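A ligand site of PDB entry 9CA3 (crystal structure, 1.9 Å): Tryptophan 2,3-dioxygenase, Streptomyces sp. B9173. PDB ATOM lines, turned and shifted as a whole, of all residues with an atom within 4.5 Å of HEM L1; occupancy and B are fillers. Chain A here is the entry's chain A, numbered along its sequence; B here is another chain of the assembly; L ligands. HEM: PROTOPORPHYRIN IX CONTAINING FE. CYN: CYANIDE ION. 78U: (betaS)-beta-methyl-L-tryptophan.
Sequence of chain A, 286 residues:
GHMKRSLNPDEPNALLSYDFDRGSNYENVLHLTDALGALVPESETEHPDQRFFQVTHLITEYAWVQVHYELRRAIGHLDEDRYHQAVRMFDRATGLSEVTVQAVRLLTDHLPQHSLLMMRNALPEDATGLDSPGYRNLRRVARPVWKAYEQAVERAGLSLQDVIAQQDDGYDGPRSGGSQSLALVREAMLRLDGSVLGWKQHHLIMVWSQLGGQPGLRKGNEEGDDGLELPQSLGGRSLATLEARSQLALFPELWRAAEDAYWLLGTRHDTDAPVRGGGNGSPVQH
NE2 of His 203 binds FE of HEM L1. NE of Arg 245 is in salt-bridge range of O2A of HEM L1, at 2.4 Å. The guanidinium group (NE) of Arg 237 lies within salt-bridge range of an oxygen (O2D) of HEM L1, 2.5 Å away. OG of Ser 233 lies within hydrogen-bond range of O2D of HEM L1, at 2.8 Å. OH of Tyr 135 is in hydrogen-bond range of O1A of HEM L1 (3.4 Å). The backbone NH (N) of Gly 129 sits at hydrogen-bond distance from a nitrogen (N) of CYN L2, at 3.0 Å. NE1 of 78U L3 sits at hydrogen-bond distance from NE2 of His 57 (3.2 Å).
N of 78U L3 is in hydrogen-bond range of N of CYN L2.
The backbone NH of Arg 237 lies within hydrogen-bond range of the side-chain hydroxyl of Ser 233. The side-chain hydroxyl (OG1) of Thr 128 sits at hydrogen-bond distance from the backbone NH (N) of Leu 130. The backbone carbonyl oxygen of Phe 53 sits at hydrogen-bond distance from a ring nitrogen (ND1) of His 57 (2.9 Å). N of Tyr 135 is in hydrogen-bond range of OG of Ser 132 (3.0 Å). The side-chain amide nitrogen (NE2) of Gln 210 is in hydrogen-bond range of the backbone carbonyl oxygen (O) of Leu 111 (2.9 Å). The side-chain hydroxyl (OG1) of Thr 60 is in hydrogen-bond range of the backbone carbonyl oxygen (O) of Thr 56 (3.0 Å). OG1 of Thr 56 sits at hydrogen-bond distance from O of Phe 53 (2.8 Å).
Thr 56 touches HEM L1. His 57 touches HEM L1. CG2 of Thr 60 touches CMB of HEM L1 (3.5 Å). Leu 107 touches HEM L1 (CD1 to CAB, 3.6 Å). Leu 116 touches HEM L1 (CD1 to CBC, 3.3 Å). Thr 128 touches HEM L1 (OG1 to CBD, 3.5 Å). Gly 129 touches HEM L1. CD2 of Leu 130 touches O2A of HEM L1 (3.2 Å). CZ2 of Trp 199 touches CHB of HEM L1 (3.5 Å). Met 206 touches HEM L1. Val 207 touches HEM L1 (CG2 to CHD, 3.4 Å). Gln 210 touches HEM L1 (CB to CBC, 3.5 Å). Leu 239 touches HEM L1 (CD2 to CMD, 3.8 Å). Thr 241 touches HEM L1. Leu 242 touches HEM L1. Hydrophobic or aromatic side chains within 4 Å of HEM L1: His 57, Leu 107, Leu 116, Leu 130, Tyr 135, Trp 199, His 203, Met 206, Val 207, Leu 239 and Leu 242. Of the 27 residues printed, 20 come within 4 Å of HEM L1.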
ATOM      1  N   PHE A  53      -1.363 -24.236   2.693  1.00  0.00           N
ATOM      2  CA  PHE A  53      -0.540 -23.962   3.860  1.00  0.00           C
ATOM      3  C   PHE A  53       0.842 -24.575   3.705  1.00  0.00           C
ATOM      4  O   PHE A  53       1.869 -23.876   3.755  1.00  0.00           O
ATOM      5  CB  PHE A  53      -1.271 -24.495   5.104  1.00  0.00           C
ATOM      6  CG  PHE A  53      -0.623 -24.160   6.427  1.00  0.00           C
ATOM      7  CD1 PHE A  53       0.287 -25.029   7.006  1.00  0.00           C
ATOM      8  CD2 PHE A  53      -0.986 -23.027   7.126  1.00  0.00           C
ATOM      9  CE1 PHE A  53       0.862 -24.744   8.229  1.00  0.00           C
ATOM     10  CE2 PHE A  53      -0.411 -22.732   8.347  1.00  0.00           C
ATOM     11  CZ  PHE A  53       0.508 -23.597   8.895  1.00  0.00           C
ATOM     12  N   THR A  56       3.252 -23.230   0.668  1.00  0.00           N
ATOM     13  CA  THR A  56       3.896 -21.934   0.849  1.00  0.00           C
ATOM     14  C   THR A  56       5.120 -22.038   1.751  1.00  0.00           C
ATOM     15  O   THR A  56       6.091 -21.305   1.552  1.00  0.00           O
ATOM     16  CB  THR A  56       2.929 -20.897   1.410  1.00  0.00           C
ATOM     17  OG1 THR A  56       2.449 -21.344   2.681  1.00  0.00           O
ATOM     18  CG2 THR A  56       1.745 -20.670   0.463  1.00  0.00           C
ATOM     19  N   HIS A  57       5.090 -22.950   2.732  1.00  0.00           N
ATOM     20  CA  HIS A  57       6.232 -23.149   3.614  1.00  0.00           C
ATOM     21  C   HIS A  57       7.358 -23.843   2.881  1.00  0.00           C
ATOM     22  O   HIS A  57       8.535 -23.474   3.011  1.00  0.00           O
ATOM     23  CB  HIS A  57       5.839 -23.982   4.835  1.00  0.00           C
ATOM     24  CG  HIS A  57       5.061 -23.243   5.866  1.00  0.00           C
ATOM     25  ND1 HIS A  57       3.690 -23.079   5.802  1.00  0.00           N
ATOM     26  CD2 HIS A  57       5.457 -22.646   7.013  1.00  0.00           C
ATOM     27  CE1 HIS A  57       3.284 -22.405   6.865  1.00  0.00           C
ATOM     28  NE2 HIS A  57       4.336 -22.130   7.618  1.00  0.00           N
ATOM     29  N   THR A  60       9.126 -21.524   0.663  1.00  0.00           N
ATOM     30  CA  THR A  60       9.955 -20.638   1.468  1.00  0.00           C
ATOM     31  C   THR A  60      11.232 -21.318   1.919  1.00  0.00           C
ATOM     32  O   THR A  60      12.315 -20.737   1.828  1.00  0.00           O
ATOM     33  CB  THR A  60       9.181 -20.137   2.687  1.00  0.00           C
ATOM     34  OG1 THR A  60       8.116 -19.257   2.273  1.00  0.00           O
ATOM     35  CG2 THR A  60      10.112 -19.388   3.627  1.00  0.00           C
ATOM     36  N   TRP A  64      15.181 -20.397   1.193  1.00  0.00           N
ATOM     37  CA  TRP A  64      16.113 -20.030   2.267  1.00  0.00           C
ATOM     38  C   TRP A  64      17.318 -20.967   2.332  1.00  0.00           C
ATOM     39  O   TRP A  64      18.431 -20.539   2.666  1.00  0.00           O
ATOM     40  CB  TRP A  64      15.390 -20.010   3.629  1.00  0.00           C
ATOM     41  CG  TRP A  64      14.748 -18.712   3.967  1.00  0.00           C
ATOM     42  CD1 TRP A  64      15.043 -17.488   3.449  1.00  0.00           C
ATOM     43  CD2 TRP A  64      13.675 -18.506   4.916  1.00  0.00           C
ATOM     44  NE1 TRP A  64      14.226 -16.531   4.021  1.00  0.00           N
ATOM     45  CE2 TRP A  64      13.385 -17.129   4.924  1.00  0.00           C
ATOM     46  CE3 TRP A  64      12.941 -19.350   5.761  1.00  0.00           C
ATOM     47  CZ2 TRP A  64      12.390 -16.574   5.732  1.00  0.00           C
ATOM     48  CZ3 TRP A  64      11.956 -18.805   6.570  1.00  0.00           C
ATOM     49  CH2 TRP A  64      11.675 -17.436   6.539  1.00  0.00           C
ATOM     50  N   VAL A 104       4.864 -15.811   1.671  1.00  0.00           N
ATOM     51  CA  VAL A 104       4.048 -15.531   2.853  1.00  0.00           C
ATOM     52  C   VAL A 104       2.916 -14.545   2.512  1.00  0.00           C
ATOM     53  O   VAL A 104       1.830 -14.612   3.105  1.00  0.00           O
ATOM     54  CB  VAL A 104       4.903 -15.060   4.042  1.00  0.00           C
ATOM     55  CG1 VAL A 104       5.429 -13.638   3.866  1.00  0.00           C
ATOM     56  CG2 VAL A 104       4.077 -15.149   5.315  1.00  0.00           C
ATOM     57  N   LEU A 107      -0.249 -16.215   1.730  1.00  0.00           N
ATOM     58  CA  LEU A 107      -1.141 -16.515   2.862  1.00  0.00           C
ATOM     59  C   LEU A 107      -1.942 -15.284   3.270  1.00  0.00           C
ATOM     60  O   LEU A 107      -3.145 -15.361   3.543  1.00  0.00           O
ATOM     61  CB  LEU A 107      -0.313 -17.024   4.037  1.00  0.00           C
ATOM     62  CG  LEU A 107       0.421 -18.340   3.821  1.00  0.00           C
ATOM     63  CD1 LEU A 107       1.053 -18.805   5.115  1.00  0.00           C
ATOM     64  CD2 LEU A 107      -0.541 -19.380   3.274  1.00  0.00           C
ATOM     65  N   LEU A 111      -5.182 -17.041   2.303  1.00  0.00           N
ATOM     66  CA  LEU A 111      -5.522 -18.034   3.329  1.00  0.00           C
ATOM     67  C   LEU A 111      -6.655 -17.489   4.193  1.00  0.00           C
ATOM     68  O   LEU A 111      -6.490 -16.441   4.823  1.00  0.00           O
ATOM     69  CB  LEU A 111      -4.301 -18.364   4.173  1.00  0.00           C
ATOM     70  CG  LEU A 111      -4.577 -19.276   5.355  1.00  0.00           C
ATOM     71  CD1 LEU A 111      -4.810 -20.673   4.866  1.00  0.00           C
ATOM     72  CD2 LEU A 111      -3.430 -19.284   6.332  1.00  0.00           C
ATOM     73  N   LEU A 116      -7.487 -21.009   8.857  1.00  0.00           N
ATOM     74  CA  LEU A 116      -6.266 -21.085   9.642  1.00  0.00           C
ATOM     75  C   LEU A 116      -6.580 -21.438  11.084  1.00  0.00           C
ATOM     76  O   LEU A 116      -5.910 -22.291  11.687  1.00  0.00           O
ATOM     77  CB  LEU A 116      -5.518 -19.750   9.547  1.00  0.00           C
ATOM     78  CG  LEU A 116      -4.177 -19.554  10.266  1.00  0.00           C
ATOM     79  CD1 LEU A 116      -4.425 -19.045  11.693  1.00  0.00           C
ATOM     80  CD2 LEU A 116      -3.356 -20.808  10.270  1.00  0.00           C
ATOM     81  N   THR A 128       6.187 -24.165  15.639  1.00  0.00           N
ATOM     82  CA  THR A 128       6.642 -22.785  15.462  1.00  0.00           C
ATOM     83  C   THR A 128       7.766 -22.729  14.442  1.00  0.00           C
ATOM     84  O   THR A 128       8.607 -23.633  14.358  1.00  0.00           O
ATOM     85  CB  THR A 128       7.172 -22.177  16.777  1.00  0.00           C
ATOM     86  OG1 THR A 128       7.884 -20.982  16.486  1.00  0.00           O
ATOM     87  CG2 THR A 128       8.145 -23.139  17.505  1.00  0.00           C
ATOM     88  N   GLY A 129       7.824 -21.620  13.697  1.00  0.00           N
ATOM     89  CA  GLY A 129       8.922 -21.353  12.769  1.00  0.00           C
ATOM     90  C   GLY A 129      10.233 -20.954  13.430  1.00  0.00           C
ATOM     91  O   GLY A 129      11.235 -20.798  12.719  1.00  0.00           O
ATOM     92  N   LEU A 130      10.250 -20.781  14.751  1.00  0.00           N
ATOM     93  CA  LEU A 130      11.529 -20.720  15.457  1.00  0.00           C
ATOM     94  C   LEU A 130      12.344 -21.986  15.239  1.00  0.00           C
ATOM     95  O   LEU A 130      13.561 -21.975  15.468  1.00  0.00           O
ATOM     96  CB  LEU A 130      11.301 -20.484  16.946  1.00  0.00           C
ATOM     97  CG  LEU A 130      10.660 -19.132  17.295  1.00  0.00           C
ATOM     98  CD1 LEU A 130      10.088 -19.134  18.707  1.00  0.00           C
ATOM     99  CD2 LEU A 130      11.674 -17.997  17.119  1.00  0.00           C
ATOM    100  N   SER A 132      12.423 -23.343  12.208  1.00  0.00           N
ATOM    101  CA  SER A 132      12.664 -23.419  10.758  1.00  0.00           C
ATOM    102  C   SER A 132      14.157 -23.591  10.515  1.00  0.00           C
ATOM    103  O   SER A 132      14.967 -22.819  11.047  1.00  0.00           O
ATOM    104  CB  SER A 132      12.155 -22.156  10.061  1.00  0.00           C
ATOM    105  OG  SER A 132      12.772 -22.003   8.802  1.00  0.00           O
ATOM    106  N   TYR A 135      15.311 -20.397   8.656  1.00  0.00           N
ATOM    107  CA  TYR A 135      15.463 -19.218   9.495  1.00  0.00           C
ATOM    108  C   TYR A 135      16.667 -19.328  10.419  1.00  0.00           C
ATOM    109  O   TYR A 135      17.496 -18.411  10.484  1.00  0.00           O
ATOM    110  CB  TYR A 135      14.195 -18.959  10.296  1.00  0.00           C
ATOM    111  CG  TYR A 135      14.323 -17.631  10.953  1.00  0.00           C
ATOM    112  CD1 TYR A 135      14.441 -16.477  10.178  1.00  0.00           C
ATOM    113  CD2 TYR A 135      14.421 -17.530  12.327  1.00  0.00           C
ATOM    114  CE1 TYR A 135      14.596 -15.241  10.782  1.00  0.00           C
ATOM    115  CE2 TYR A 135      14.586 -16.294  12.930  1.00  0.00           C
ATOM    116  CZ  TYR A 135      14.664 -15.160  12.160  1.00  0.00           C
ATOM    117  OH  TYR A 135      14.829 -13.924  12.763  1.00  0.00           O
ATOM    118  N   TRP A 199      10.594  -9.428   4.642  1.00  0.00           N
ATOM    119  CA  TRP A 199       9.954 -10.690   5.005  1.00  0.00           C
ATOM    120  C   TRP A 199       9.392 -10.632   6.415  1.00  0.00           C
ATOM    121  O   TRP A 199       8.245 -10.991   6.649  1.00  0.00           O
ATOM    122  CB  TRP A 199      10.902 -11.889   4.872  1.00  0.00           C
ATOM    123  CG  TRP A 199      10.152 -13.169   5.252  1.00  0.00           C
ATOM    124  CD1 TRP A 199       9.413 -13.963   4.396  1.00  0.00           C
ATOM    125  CD2 TRP A 199      10.003 -13.752   6.560  1.00  0.00           C
ATOM    126  NE1 TRP A 199       8.833 -14.999   5.091  1.00  0.00           N
ATOM    127  CE2 TRP A 199       9.190 -14.908   6.418  1.00  0.00           C
ATOM    128  CE3 TRP A 199      10.479 -13.427   7.829  1.00  0.00           C
ATOM    129  CZ2 TRP A 199       8.843 -15.727   7.502  1.00  0.00           C
ATOM    130  CZ3 TRP A 199      10.142 -14.237   8.911  1.00  0.00           C
ATOM    131  CH2 TRP A 199       9.328 -15.369   8.734  1.00  0.00           C
ATOM    132  N   HIS A 203       5.448 -11.044   7.186  1.00  0.00           N
ATOM    133  CA  HIS A 203       5.042 -12.152   8.042  1.00  0.00           C
ATOM    134  C   HIS A 203       4.278 -11.641   9.260  1.00  0.00           C
ATOM    135  O   HIS A 203       3.295 -12.260   9.681  1.00  0.00           O
ATOM    136  CB  HIS A 203       6.288 -12.929   8.462  1.00  0.00           C
ATOM    137  CG  HIS A 203       5.996 -14.036   9.427  1.00  0.00           C
ATOM    138  ND1 HIS A 203       6.044 -13.854  10.797  1.00  0.00           N
ATOM    139  CD2 HIS A 203       5.621 -15.316   9.226  1.00  0.00           C
ATOM    140  CE1 HIS A 203       5.731 -14.992  11.391  1.00  0.00           C
ATOM    141  NE2 HIS A 203       5.469 -15.883  10.460  1.00  0.00           N
ATOM    142  N   MET A 206       0.744 -10.503   8.091  1.00  0.00           N
ATOM    143  CA  MET A 206      -0.006 -11.760   8.059  1.00  0.00           C
ATOM    144  C   MET A 206      -0.522 -12.174   9.447  1.00  0.00           C
ATOM    145  O   MET A 206      -1.720 -12.392   9.624  1.00  0.00           O
ATOM    146  CB  MET A 206       0.880 -12.861   7.481  1.00  0.00           C
ATOM    147  CG  MET A 206       0.168 -14.119   7.020  1.00  0.00           C
ATOM    148  SD  MET A 206       0.240 -15.182   8.486  1.00  0.00           S
ATOM    149  CE  MET A 206       2.018 -15.464   8.469  1.00  0.00           C
ATOM    150  N   VAL A 207       0.383 -12.294  10.422  1.00  0.00           N
ATOM    151  CA  VAL A 207      -0.024 -12.728  11.760  1.00  0.00           C
ATOM    152  C   VAL A 207      -1.134 -11.837  12.302  1.00  0.00           C
ATOM    153  O   VAL A 207      -2.112 -12.322  12.892  1.00  0.00           O
ATOM    154  CB  VAL A 207       1.191 -12.764  12.700  1.00  0.00           C
ATOM    155  CG1 VAL A 207       0.730 -12.739  14.145  1.00  0.00           C
ATOM    156  CG2 VAL A 207       1.995 -14.018  12.440  1.00  0.00           C
ATOM    157  N   GLN A 210      -4.409 -12.912  10.962  1.00  0.00           N
ATOM    158  CA  GLN A 210      -4.772 -14.296  11.228  1.00  0.00           C
ATOM    159  C   GLN A 210      -4.945 -14.604  12.698  1.00  0.00           C
ATOM    160  O   GLN A 210      -5.861 -15.335  13.068  1.00  0.00           O
ATOM    161  CB  GLN A 210      -3.725 -15.231  10.614  1.00  0.00           C
ATOM    162  CG  GLN A 210      -3.555 -15.067   9.090  1.00  0.00           C
ATOM    163  CD  GLN A 210      -4.612 -15.865   8.316  1.00  0.00           C
ATOM    164  OE1 GLN A 210      -5.028 -16.928   8.767  1.00  0.00           O
ATOM    165  NE2 GLN A 210      -5.049 -15.365   7.152  1.00  0.00           N
ATOM    166  N   LEU A 211      -4.078 -14.073  13.559  1.00  0.00           N
ATOM    167  CA  LEU A 211      -4.201 -14.254  15.003  1.00  0.00           C
ATOM    168  C   LEU A 211      -4.642 -13.002  15.733  1.00  0.00           C
ATOM    169  O   LEU A 211      -5.031 -13.092  16.902  1.00  0.00           O
ATOM    170  CB  LEU A 211      -2.868 -14.745  15.590  1.00  0.00           C
ATOM    171  CG  LEU A 211      -2.342 -16.086  15.079  1.00  0.00           C
ATOM    172  CD1 LEU A 211      -1.152 -16.529  15.915  1.00  0.00           C
ATOM    173  CD2 LEU A 211      -3.430 -17.151  15.091  1.00  0.00           C
ATOM    174  N   SER A 233       1.230 -17.562  20.366  1.00  0.00           N
ATOM    175  CA  SER A 233       1.678 -18.585  19.450  1.00  0.00           C
ATOM    176  C   SER A 233       1.261 -19.977  19.933  1.00  0.00           C
ATOM    177  O   SER A 233       0.718 -20.154  21.022  1.00  0.00           O
ATOM    178  CB  SER A 233       3.206 -18.515  19.302  1.00  0.00           C
ATOM    179  OG  SER A 233       3.859 -19.200  20.352  1.00  0.00           O
ATOM    180  N   ARG A 237       3.553 -18.101  23.572  1.00  0.00           N
ATOM    181  CA  ARG A 237       4.246 -16.819  23.683  1.00  0.00           C
ATOM    182  C   ARG A 237       3.437 -15.696  23.052  1.00  0.00           C
ATOM    183  O   ARG A 237       2.768 -15.891  22.029  1.00  0.00           O
ATOM    184  CB  ARG A 237       5.639 -16.886  23.035  1.00  0.00           C
ATOM    185  CG  ARG A 237       6.578 -17.927  23.667  1.00  0.00           C
ATOM    186  CD  ARG A 237       7.793 -18.242  22.787  1.00  0.00           C
ATOM    187  NE  ARG A 237       7.467 -19.206  21.739  1.00  0.00           N
ATOM    188  CZ  ARG A 237       7.898 -20.453  21.722  1.00  0.00           C
ATOM    189  NH1 ARG A 237       8.700 -20.923  22.676  1.00  0.00           N
ATOM    190  NH2 ARG A 237       7.515 -21.263  20.737  1.00  0.00           N
ATOM    191  N   LEU A 239       2.417 -12.339  21.009  1.00  0.00           N
ATOM    192  CA  LEU A 239       2.786 -11.795  19.712  1.00  0.00           C
ATOM    193  C   LEU A 239       3.739 -10.615  19.825  1.00  0.00           C
ATOM    194  O   LEU A 239       4.335 -10.218  18.825  1.00  0.00           O
ATOM    195  CB  LEU A 239       1.519 -11.364  18.972  1.00  0.00           C
ATOM    196  CG  LEU A 239       0.561 -12.510  18.619  1.00  0.00           C
ATOM    197  CD1 LEU A 239      -0.453 -12.032  17.598  1.00  0.00           C
ATOM    198  CD2 LEU A 239       1.338 -13.704  18.083  1.00  0.00           C
ATOM    199  N   THR A 241       6.552 -10.658  21.435  1.00  0.00           N
ATOM    200  CA  THR A 241       7.894 -11.179  21.232  1.00  0.00           C
ATOM    201  C   THR A 241       8.193 -11.311  19.752  1.00  0.00           C
ATOM    202  O   THR A 241       9.304 -11.003  19.304  1.00  0.00           O
ATOM    203  CB  THR A 241       8.073 -12.519  21.943  1.00  0.00           C
ATOM    204  OG1 THR A 241       7.161 -13.469  21.388  1.00  0.00           O
ATOM    205  CG2 THR A 241       7.834 -12.363  23.438  1.00  0.00           C
ATOM    206  N   LEU A 242       7.209 -11.745  18.966  1.00  0.00           N
ATOM    207  CA  LEU A 242       7.379 -11.801  17.516  1.00  0.00           C
ATOM    208  C   LEU A 242       7.685 -10.411  16.965  1.00  0.00           C
ATOM    209  O   LEU A 242       8.615 -10.241  16.162  1.00  0.00           O
ATOM    210  CB  LEU A 242       6.137 -12.385  16.848  1.00  0.00           C
ATOM    211  CG  LEU A 242       6.206 -12.433  15.327  1.00  0.00           C
ATOM    212  CD1 LEU A 242       7.326 -13.383  14.847  1.00  0.00           C
ATOM    213  CD2 LEU A 242       4.866 -12.814  14.705  1.00  0.00           C
ATOM    214  N   ARG A 245      11.394  -9.403  17.695  1.00  0.00           N
ATOM    215  CA  ARG A 245      12.356 -10.069  16.838  1.00  0.00           C
ATOM    216  C   ARG A 245      12.230  -9.645  15.385  1.00  0.00           C
ATOM    217  O   ARG A 245      13.147  -9.911  14.595  1.00  0.00           O
ATOM    218  CB  ARG A 245      12.197 -11.577  16.939  1.00  0.00           C
ATOM    219  CG  ARG A 245      12.758 -12.135  18.223  1.00  0.00           C
ATOM    220  CD  ARG A 245      12.855 -13.644  18.164  1.00  0.00           C
ATOM    221  NE  ARG A 245      11.579 -14.210  17.748  1.00  0.00           N
ATOM    222  CZ  ARG A 245      10.619 -14.563  18.597  1.00  0.00           C
ATOM    223  NH1 ARG A 245      10.775 -14.435  19.903  1.00  0.00           N
ATOM    224  NH2 ARG A 245       9.472 -15.059  18.124  1.00  0.00           N
ATOM    225  N   TYR B  26       7.153 -28.191  13.992  1.00  0.00           N
ATOM    226  CA  TYR B  26       7.135 -27.443  12.748  1.00  0.00           C
ATOM    227  C   TYR B  26       7.689 -28.274  11.609  1.00  0.00           C
ATOM    228  O   TYR B  26       7.109 -28.340  10.517  1.00  0.00           O
ATOM    229  CB  TYR B  26       7.950 -26.160  12.916  1.00  0.00           C
ATOM    230  CG  TYR B  26       8.202 -25.366  11.646  1.00  0.00           C
ATOM    231  CD1 TYR B  26       9.277 -25.672  10.809  1.00  0.00           C
ATOM    232  CD2 TYR B  26       7.380 -24.288  11.309  1.00  0.00           C
ATOM    233  CE1 TYR B  26       9.512 -24.938   9.652  1.00  0.00           C
ATOM    234  CE2 TYR B  26       7.605 -23.552  10.163  1.00  0.00           C
ATOM    235  CZ  TYR B  26       8.671 -23.888   9.331  1.00  0.00           C
ATOM    236  OH  TYR B  26       8.886 -23.150   8.195  1.00  0.00           O
HETATM  237  CHA HEM L   1       7.332 -17.280  13.915  1.00  0.00           C
HETATM  238  CHB HEM L   1       8.180 -18.641   9.335  1.00  0.00           C
HETATM  239  CHC HEM L   1       3.376 -18.654   8.525  1.00  0.00           C
HETATM  240  CHD HEM L   1       2.558 -17.288  13.073  1.00  0.00           C
HETATM  241  C1A HEM L   1       7.968 -17.580  12.732  1.00  0.00           C
HETATM  242  C2A HEM L   1       9.394 -17.493  12.513  1.00  0.00           C
HETATM  243  C3A HEM L   1       9.617 -17.868  11.254  1.00  0.00           C
HETATM  244  C4A HEM L   1       8.358 -18.209  10.632  1.00  0.00           C
HETATM  245  CMA HEM L   1      10.968 -17.940  10.527  1.00  0.00           C
HETATM  246  CAA HEM L   1      10.426 -17.018  13.564  1.00  0.00           C
HETATM  247  CBA HEM L   1      10.797 -15.581  13.205  1.00  0.00           C
HETATM  248  CGA HEM L   1      11.275 -14.754  14.388  1.00  0.00           C
HETATM  249  O1A HEM L   1      11.768 -13.618  14.155  1.00  0.00           O
HETATM  250  O2A HEM L   1      11.153 -15.210  15.559  1.00  0.00           O
HETATM  251  C1B HEM L   1       6.942 -18.747   8.718  1.00  0.00           C
HETATM  252  C2B HEM L   1       6.702 -19.065   7.329  1.00  0.00           C
HETATM  253  C3B HEM L   1       5.367 -19.059   7.131  1.00  0.00           C
HETATM  254  C4B HEM L   1       4.742 -18.726   8.378  1.00  0.00           C
HETATM  255  CMB HEM L   1       7.834 -19.362   6.325  1.00  0.00           C
HETATM  256  CAB HEM L   1       4.530 -19.324   5.850  1.00  0.00           C
HETATM  257  CBB HEM L   1       5.047 -19.358   4.620  1.00  0.00           C
HETATM  258  C1C HEM L   1       2.709 -18.337   9.685  1.00  0.00           C
HETATM  259  C2C HEM L   1       1.274 -18.326   9.886  1.00  0.00           C
HETATM  260  C3C HEM L   1       1.081 -17.938  11.162  1.00  0.00           C
HETATM  261  C4C HEM L   1       2.360 -17.701  11.773  1.00  0.00           C
HETATM  262  CMC HEM L   1       0.222 -18.704   8.807  1.00  0.00           C
HETATM  263  CAC HEM L   1      -0.216 -17.737  11.975  1.00  0.00           C
HETATM  264  CBC HEM L   1      -1.412 -17.703  11.401  1.00  0.00           C
HETATM  265  C1D HEM L   1       3.796 -17.190  13.702  1.00  0.00           C
HETATM  266  C2D HEM L   1       4.006 -16.861  15.100  1.00  0.00           C
HETATM  267  C3D HEM L   1       5.313 -16.857  15.348  1.00  0.00           C
HETATM  268  C4D HEM L   1       5.977 -17.180  14.097  1.00  0.00           C
HETATM  269  CMD HEM L   1       2.864 -16.585  16.098  1.00  0.00           C
HETATM  270  CAD HEM L   1       6.011 -16.570  16.689  1.00  0.00           C
HETATM  271  CBD HEM L   1       6.458 -17.901  17.289  1.00  0.00           C
HETATM  272  CGD HEM L   1       6.738 -17.740  18.768  1.00  0.00           C
HETATM  273  O1D HEM L   1       7.208 -16.644  19.175  1.00  0.00           O
HETATM  274  O2D HEM L   1       6.512 -18.712  19.532  1.00  0.00           O
HETATM  275  NA  HEM L   1       7.364 -18.026  11.572  1.00  0.00           N
HETATM  276  NB  HEM L   1       5.729 -18.546   9.324  1.00  0.00           N
HETATM  277  NC  HEM L   1       3.343 -17.953  10.846  1.00  0.00           N
HETATM  278  ND  HEM L   1       5.019 -17.376  13.123  1.00  0.00           N
HETATM  279 FE   HEM L   1       5.355 -18.026  11.282  1.00  0.00          FE
HETATM  280  C   CYN L   2       5.499 -20.112  11.608  1.00  0.00           C
HETATM  281  N   CYN L   2       5.192 -20.582  12.604  1.00  0.00           N
HETATM  282  OXT 78U L   3       2.068 -20.491  16.586  1.00  0.00           O
HETATM  283  C   78U L   3       1.410 -20.380  15.514  1.00  0.00           C
HETATM  284  O   78U L   3       0.283 -19.848  15.515  1.00  0.00           O
HETATM  285  CA  78U L   3       2.031 -20.869  14.195  1.00  0.00           C
HETATM  286  N   78U L   3       3.336 -21.413  14.507  1.00  0.00           N
HETATM  287  CB  78U L   3       1.155 -21.923  13.526  1.00  0.00           C
HETATM  288  CAG 78U L   3      -0.060 -21.291  12.827  1.00  0.00           C
HETATM  289  CG  78U L   3       2.002 -22.693  12.499  1.00  0.00           C
HETATM  290  CD2 78U L   3       2.632 -23.816  12.065  1.00  0.00           C
HETATM  291  CE3 78U L   3       2.738 -25.102  12.636  1.00  0.00           C
HETATM  292  CZ3 78U L   3       3.443 -26.077  11.968  1.00  0.00           C
HETATM  293  CH2 78U L   3       4.043 -25.794  10.746  1.00  0.00           C
HETATM  294  CZ2 78U L   3       3.927 -24.526  10.189  1.00  0.00           C
HETATM  295  CE2 78U L   3       3.243 -23.538  10.874  1.00  0.00           C
HETATM  296  NE1 78U L   3       2.963 -22.225  10.548  1.00  0.00           N
HETATM  297  CD1 78U L   3       2.204 -21.705  11.549  1.00  0.00           C
